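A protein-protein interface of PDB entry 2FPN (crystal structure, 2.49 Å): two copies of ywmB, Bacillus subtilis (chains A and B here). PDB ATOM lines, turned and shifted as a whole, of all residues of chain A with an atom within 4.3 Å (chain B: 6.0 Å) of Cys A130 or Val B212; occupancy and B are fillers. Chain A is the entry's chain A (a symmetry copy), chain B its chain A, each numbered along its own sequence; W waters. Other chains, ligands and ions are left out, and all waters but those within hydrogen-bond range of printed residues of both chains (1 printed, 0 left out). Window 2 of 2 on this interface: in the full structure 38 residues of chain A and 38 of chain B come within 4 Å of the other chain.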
ATOM      1  N   LYS A  20      19.126  30.916 -39.704  1.00  0.00           N
ATOM      2  CA  LYS A  20      18.825  29.577 -39.210  1.00  0.00           C
ATOM      3  C   LYS A  20      18.077  29.662 -37.891  1.00  0.00           C
ATOM      4  O   LYS A  20      18.428  30.450 -37.017  1.00  0.00           O
ATOM      5  CB  LYS A  20      20.140  28.804 -39.033  1.00  0.00           C
ATOM      6  CG  LYS A  20      20.100  27.520 -38.217  1.00  0.00           C
ATOM      7  CD  LYS A  20      21.334  26.701 -38.531  1.00  0.00           C
ATOM      8  CE  LYS A  20      21.888  26.041 -37.289  1.00  0.00           C
ATOM      9  NZ  LYS A  20      22.973  25.080 -37.640  1.00  0.00           N
ATOM     10  N   TRP A  21      17.033  28.858 -37.753  1.00  0.00           N
ATOM     11  CA  TRP A  21      16.394  28.665 -36.447  1.00  0.00           C
ATOM     12  C   TRP A  21      16.408  27.202 -36.082  1.00  0.00           C
ATOM     13  O   TRP A  21      16.357  26.347 -36.958  1.00  0.00           O
ATOM     14  CB  TRP A  21      14.967  29.180 -36.438  1.00  0.00           C
ATOM     15  CG  TRP A  21      14.162  28.723 -37.587  1.00  0.00           C
ATOM     16  CD1 TRP A  21      14.135  29.271 -38.848  1.00  0.00           C
ATOM     17  CD2 TRP A  21      13.231  27.626 -37.600  1.00  0.00           C
ATOM     18  NE1 TRP A  21      13.250  28.568 -39.642  1.00  0.00           N
ATOM     19  CE2 TRP A  21      12.678  27.563 -38.899  1.00  0.00           C
ATOM     20  CE3 TRP A  21      12.815  26.691 -36.639  1.00  0.00           C
ATOM     21  CZ2 TRP A  21      11.734  26.599 -39.263  1.00  0.00           C
ATOM     22  CZ3 TRP A  21      11.864  25.749 -36.994  1.00  0.00           C
ATOM     23  CH2 TRP A  21      11.342  25.697 -38.295  1.00  0.00           C
ATOM     24  N   THR A  22      16.511  26.906 -34.792  1.00  0.00           N
ATOM     25  CA  THR A  22      16.321  25.542 -34.366  1.00  0.00           C
ATOM     26  C   THR A  22      15.519  25.459 -33.074  1.00  0.00           C
ATOM     27  O   THR A  22      15.661  26.317 -32.199  1.00  0.00           O
ATOM     28  CB  THR A  22      17.634  24.723 -34.270  1.00  0.00           C
ATOM     29  OG1 THR A  22      17.908  24.410 -32.909  1.00  0.00           O
ATOM     30  CG2 THR A  22      18.839  25.439 -34.888  1.00  0.00           C
ATOM     31  N   PHE A 128      13.586  24.310 -26.260  1.00  0.00           N
ATOM     32  CA  PHE A 128      14.663  25.265 -26.444  1.00  0.00           C
ATOM     33  C   PHE A 128      14.632  25.894 -27.833  1.00  0.00           C
ATOM     34  O   PHE A 128      14.647  25.191 -28.831  1.00  0.00           O
ATOM     35  CB  PHE A 128      16.008  24.584 -26.253  1.00  0.00           C
ATOM     36  CG  PHE A 128      16.308  24.180 -24.836  1.00  0.00           C
ATOM     37  CD1 PHE A 128      15.694  23.060 -24.260  1.00  0.00           C
ATOM     38  CD2 PHE A 128      17.258  24.873 -24.096  1.00  0.00           C
ATOM     39  CE1 PHE A 128      15.988  22.666 -22.961  1.00  0.00           C
ATOM     40  CE2 PHE A 128      17.570  24.475 -22.772  1.00  0.00           C
ATOM     41  CZ  PHE A 128      16.932  23.378 -22.215  1.00  0.00           C
ATOM     42  N   THR A 129      14.627  27.223 -27.876  1.00  0.00           N
ATOM     43  CA  THR A 129      14.632  27.981 -29.126  1.00  0.00           C
ATOM     44  C   THR A 129      15.956  28.716 -29.316  1.00  0.00           C
ATOM     45  O   THR A 129      16.438  29.383 -28.393  1.00  0.00           O
ATOM     46  CB  THR A 129      13.504  29.013 -29.146  1.00  0.00           C
ATOM     47  OG1 THR A 129      12.263  28.379 -28.799  1.00  0.00           O
ATOM     48  CG2 THR A 129      13.384  29.626 -30.515  1.00  0.00           C
ATOM     49  N   CYS A 130      16.526  28.601 -30.515  1.00  0.00           N
ATOM     50  CA  CYS A 130      17.785  29.259 -30.842  1.00  0.00           C
ATOM     51  C   CYS A 130      17.788  29.760 -32.273  1.00  0.00           C
ATOM     52  O   CYS A 130      17.583  28.996 -33.211  1.00  0.00           O
ATOM     53  CB  CYS A 130      18.965  28.309 -30.627  1.00  0.00           C
ATOM     54  SG  CYS A 130      20.603  29.025 -31.014  1.00  0.00           S
ATOM     55  N   LEU A 131      18.030  31.057 -32.430  1.00  0.00           N
ATOM     56  CA  LEU A 131      18.155  31.677 -33.749  1.00  0.00           C
ATOM     57  C   LEU A 131      19.605  32.109 -34.041  1.00  0.00           C
ATOM     58  O   LEU A 131      20.332  32.591 -33.156  1.00  0.00           O
ATOM     59  CB  LEU A 131      17.247  32.896 -33.862  1.00  0.00           C
ATOM     60  CG  LEU A 131      15.712  32.948 -33.893  1.00  0.00           C
ATOM     61  CD1 LEU A 131      15.154  32.330 -35.141  1.00  0.00           C
ATOM     62  CD2 LEU A 131      15.032  32.394 -32.650  1.00  0.00           C
ATOM     63  N   GLN B 191      19.843  34.170 -23.807  1.00  0.00           N
ATOM     64  CA  GLN B 191      21.261  34.344 -24.149  1.00  0.00           C
ATOM     65  C   GLN B 191      21.430  35.012 -25.515  1.00  0.00           C
ATOM     66  O   GLN B 191      20.969  34.481 -26.535  1.00  0.00           O
ATOM     67  CB  GLN B 191      22.026  33.012 -24.127  1.00  0.00           C
ATOM     68  CG  GLN B 191      22.946  32.796 -22.913  1.00  0.00           C
ATOM     69  CD  GLN B 191      23.301  31.312 -22.680  1.00  0.00           C
ATOM     70  OE1 GLN B 191      23.426  30.527 -23.625  1.00  0.00           O
ATOM     71  NE2 GLN B 191      23.469  30.933 -21.412  1.00  0.00           N
ATOM     72  N   ILE B 192      22.087  36.178 -25.507  1.00  0.00           N
ATOM     73  CA  ILE B 192      22.470  36.927 -26.707  1.00  0.00           C
ATOM     74  C   ILE B 192      23.975  36.788 -26.918  1.00  0.00           C
ATOM     75  O   ILE B 192      24.747  36.958 -25.974  1.00  0.00           O
ATOM     76  CB  ILE B 192      22.197  38.445 -26.542  1.00  0.00           C
ATOM     77  CG1 ILE B 192      20.864  38.715 -25.821  1.00  0.00           C
ATOM     78  CG2 ILE B 192      22.302  39.162 -27.880  1.00  0.00           C
ATOM     79  CD1 ILE B 192      19.627  38.705 -26.701  1.00  0.00           C
ATOM     80  N   ALA B 193      24.392  36.499 -28.151  1.00  0.00           N
ATOM     81  CA  ALA B 193      25.816  36.333 -28.460  1.00  0.00           C
ATOM     82  C   ALA B 193      26.208  36.845 -29.850  1.00  0.00           C
ATOM     83  O   ALA B 193      25.716  36.349 -30.869  1.00  0.00           O
ATOM     84  CB  ALA B 193      26.251  34.876 -28.269  1.00  0.00           C
ATOM     85  N   THR B 206      23.529  35.302 -32.217  1.00  0.00           N
ATOM     86  CA  THR B 206      22.868  34.113 -31.677  1.00  0.00           C
ATOM     87  C   THR B 206      21.976  34.463 -30.493  1.00  0.00           C
ATOM     88  O   THR B 206      22.433  35.045 -29.515  1.00  0.00           O
ATOM     89  CB  THR B 206      23.870  33.016 -31.270  1.00  0.00           C
ATOM     90  OG1 THR B 206      24.835  32.837 -32.313  1.00  0.00           O
ATOM     91  CG2 THR B 206      23.149  31.690 -31.050  1.00  0.00           C
ATOM     92  N   VAL B 207      20.702  34.094 -30.603  1.00  0.00           N
ATOM     93  CA  VAL B 207      19.682  34.398 -29.600  1.00  0.00           C
ATOM     94  C   VAL B 207      18.926  33.102 -29.203  1.00  0.00           C
ATOM     95  O   VAL B 207      18.400  32.402 -30.066  1.00  0.00           O
ATOM     96  CB  VAL B 207      18.701  35.488 -30.128  1.00  0.00           C
ATOM     97  CG1 VAL B 207      17.838  36.030 -29.017  1.00  0.00           C
ATOM     98  CG2 VAL B 207      19.457  36.640 -30.773  1.00  0.00           C
ATOM     99  N   GLY B 208      18.877  32.804 -27.901  1.00  0.00           N
ATOM    100  CA  GLY B 208      18.389  31.518 -27.396  1.00  0.00           C
ATOM    101  C   GLY B 208      17.601  31.530 -26.088  1.00  0.00           C
ATOM    102  O   GLY B 208      17.834  32.378 -25.224  1.00  0.00           O
ATOM    103  N   THR B 209      16.667  30.575 -25.953  1.00  0.00           N
ATOM    104  CA  THR B 209      15.806  30.415 -24.766  1.00  0.00           C
ATOM    105  C   THR B 209      15.722  28.955 -24.348  1.00  0.00           C
ATOM    106  O   THR B 209      15.425  28.106 -25.181  1.00  0.00           O
ATOM    107  CB  THR B 209      14.326  30.772 -25.056  1.00  0.00           C
ATOM    108  OG1 THR B 209      14.237  31.974 -25.825  1.00  0.00           O
ATOM    109  CG2 THR B 209      13.518  30.905 -23.752  1.00  0.00           C
ATOM    110  N   PRO B 210      15.943  28.664 -23.054  1.00  0.00           N
ATOM    111  CA  PRO B 210      16.536  29.528 -22.028  1.00  0.00           C
ATOM    112  C   PRO B 210      18.030  29.857 -22.212  1.00  0.00           C
ATOM    113  O   PRO B 210      18.458  30.942 -21.821  1.00  0.00           O
ATOM    114  CB  PRO B 210      16.310  28.739 -20.735  1.00  0.00           C
ATOM    115  CG  PRO B 210      15.200  27.784 -21.054  1.00  0.00           C
ATOM    116  CD  PRO B 210      15.453  27.407 -22.469  1.00  0.00           C
ATOM    117  N   ILE B 211      18.809  28.925 -22.769  1.00  0.00           N
ATOM    118  CA  ILE B 211      20.215  29.176 -23.129  1.00  0.00           C
ATOM    119  C   ILE B 211      20.508  28.705 -24.554  1.00  0.00           C
ATOM    120  O   ILE B 211      19.820  27.813 -25.066  1.00  0.00           O
ATOM    121  CB  ILE B 211      21.264  28.524 -22.136  1.00  0.00           C
ATOM    122  CG1 ILE B 211      21.533  27.039 -22.435  1.00  0.00           C
ATOM    123  CG2 ILE B 211      20.904  28.776 -20.682  1.00  0.00           C
ATOM    124  CD1 ILE B 211      20.774  26.049 -21.553  1.00  0.00           C
ATOM    125  N   VAL B 212      21.513  29.306 -25.201  1.00  0.00           N
ATOM    126  CA  VAL B 212      22.068  28.704 -26.426  1.00  0.00           C
ATOM    127  C   VAL B 212      23.025  27.543 -26.074  1.00  0.00           C
ATOM    128  O   VAL B 212      24.097  27.762 -25.499  1.00  0.00           O
ATOM    129  CB  VAL B 212      22.682  29.733 -27.439  1.00  0.00           C
ATOM    130  CG1 VAL B 212      23.608  30.747 -26.760  1.00  0.00           C
ATOM    131  CG2 VAL B 212      23.402  28.999 -28.587  1.00  0.00           C
ATOM    132  N   THR B 213      22.605  26.317 -26.414  1.00  0.00           N
ATOM    133  CA  THR B 213      23.318  25.080 -26.058  1.00  0.00           C
ATOM    134  C   THR B 213      24.393  24.632 -27.075  1.00  0.00           C
ATOM    135  O   THR B 213      24.864  25.440 -27.901  1.00  0.00           O
ATOM    136  CB  THR B 213      22.321  23.927 -25.815  1.00  0.00           C
ATOM    137  OG1 THR B 213      21.144  24.148 -26.600  1.00  0.00           O
ATOM    138  CG2 THR B 213      21.927  23.850 -24.351  1.00  0.00           C
ATOM    139  N   THR B 214      24.773  23.345 -26.989  1.00  0.00           N
ATOM    140  CA  THR B 214      25.857  22.734 -27.786  1.00  0.00           C
ATOM    141  C   THR B 214      25.834  21.197 -27.718  1.00  0.00           C
ATOM    142  O   THR B 214      24.953  20.542 -28.279  1.00  0.00           O
ATOM    143  CB  THR B 214      27.272  23.245 -27.338  1.00  0.00           C
ATOM    144  OG1 THR B 214      28.239  22.960 -28.364  1.00  0.00           O
ATOM    145  CG2 THR B 214      27.721  22.596 -26.004  1.00  0.00           C
HETATM  146  O   HOH W   1      18.875  27.089 -27.844  1.00  0.00           O
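The backbone NH (N) of Thr A22 lies within hydrogen-bond range of the backbone carbonyl oxygen (O) of Cys A130 (2.8 Å). OE1 of Gln B191 is in hydrogen-bond range of N of Val B212 (2.8 Å). The backbone NH of Gly B208 is in hydrogen-bond range of the backbone carbonyl oxygen of Gln B191 (3.0 Å). The backbone carbonyl oxygen (O) of Ala B193 lies within hydrogen-bond range of the backbone NH (N) of Thr B206 (2.8 Å).
The backbone NH (N) of Thr B209 sits at hydrogen-bond distance from the backbone carbonyl oxygen (O) of Thr A129, at 2.7 Å. The backbone carbonyl oxygen (O) of Val B207 sits at hydrogen-bond distance from the backbone NH (N) of Leu A131 (2.7 Å).
CA of Phe A128 touches O of Thr B209, 3.2 Å away. CD2 of Phe A128 touches CD of Pro B210, 3.5 Å away. Ile B211 touches Phe A128 (CD1 to CE2, 3.8 Å). Thr A129 touches Val B207. Thr A129 touches Gly B208. Thr B206 touches Cys A130 (CG2 to SG, 3.7 Å). Val B207 touches Cys A130. SG of Cys A130 touches CG2 of Val B212 (3.7 Å). Thr B206 touches Leu A131 (CA to O, 3.3 Å).
Of the 12 printed residues of chain B, 7 touch a printed residue of chain A. Along chain B the printed residues that touch a printed residue of chain A span positions 206 to 212. Hydrophobic or aromatic side chains of chain A within 4 Å of the printed part of chain B: Phe A128 and Leu A131. Among the printed residues, 11 pairs touch across the chains.
Of the printed residues of chain B, Thr A129 touches Val B207 (3.97 Å), Gly B208 (3.1 Å) and Thr B209 (2.7 Å). Of the printed residues of chain A, Thr B206 touches Cys A130 (3.7 Å) and Leu A131 (3.3 Å). Printed residues of chain A within 4 Å of Val B207: Thr A129, Cys A130 and Leu A131. Of the printed residues of chain A, Gly B208 touches Thr A129 (3.1 Å). Of the printed residues of chain A, Pro B210 touches Phe A128 (3.5 Å). Val B212 touches just one residue of chain A: Cys A130 (3.7 Å). The nearest residue of chain B that does not touch Cys A130 is Gly B208 (4.2 Å). The nearest printed residue of chain A that does not touch Val B212 is Thr A129 (6.0 Å). The nearest printed residue of chain A that does not touch Gly B208 is Cys A130 (4.2 Å).
Water W1 lies within hydrogen-bond range of the backbone carbonyl oxygen of Ile B211 (3.0 Å) and the backbone carbonyl oxygen of Thr A129 (3.4 Å).
No position is printed for both chains. Of the 11 pairs that touch across the chains among the printed residues, none has its exchanged pair printed and touching as well.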
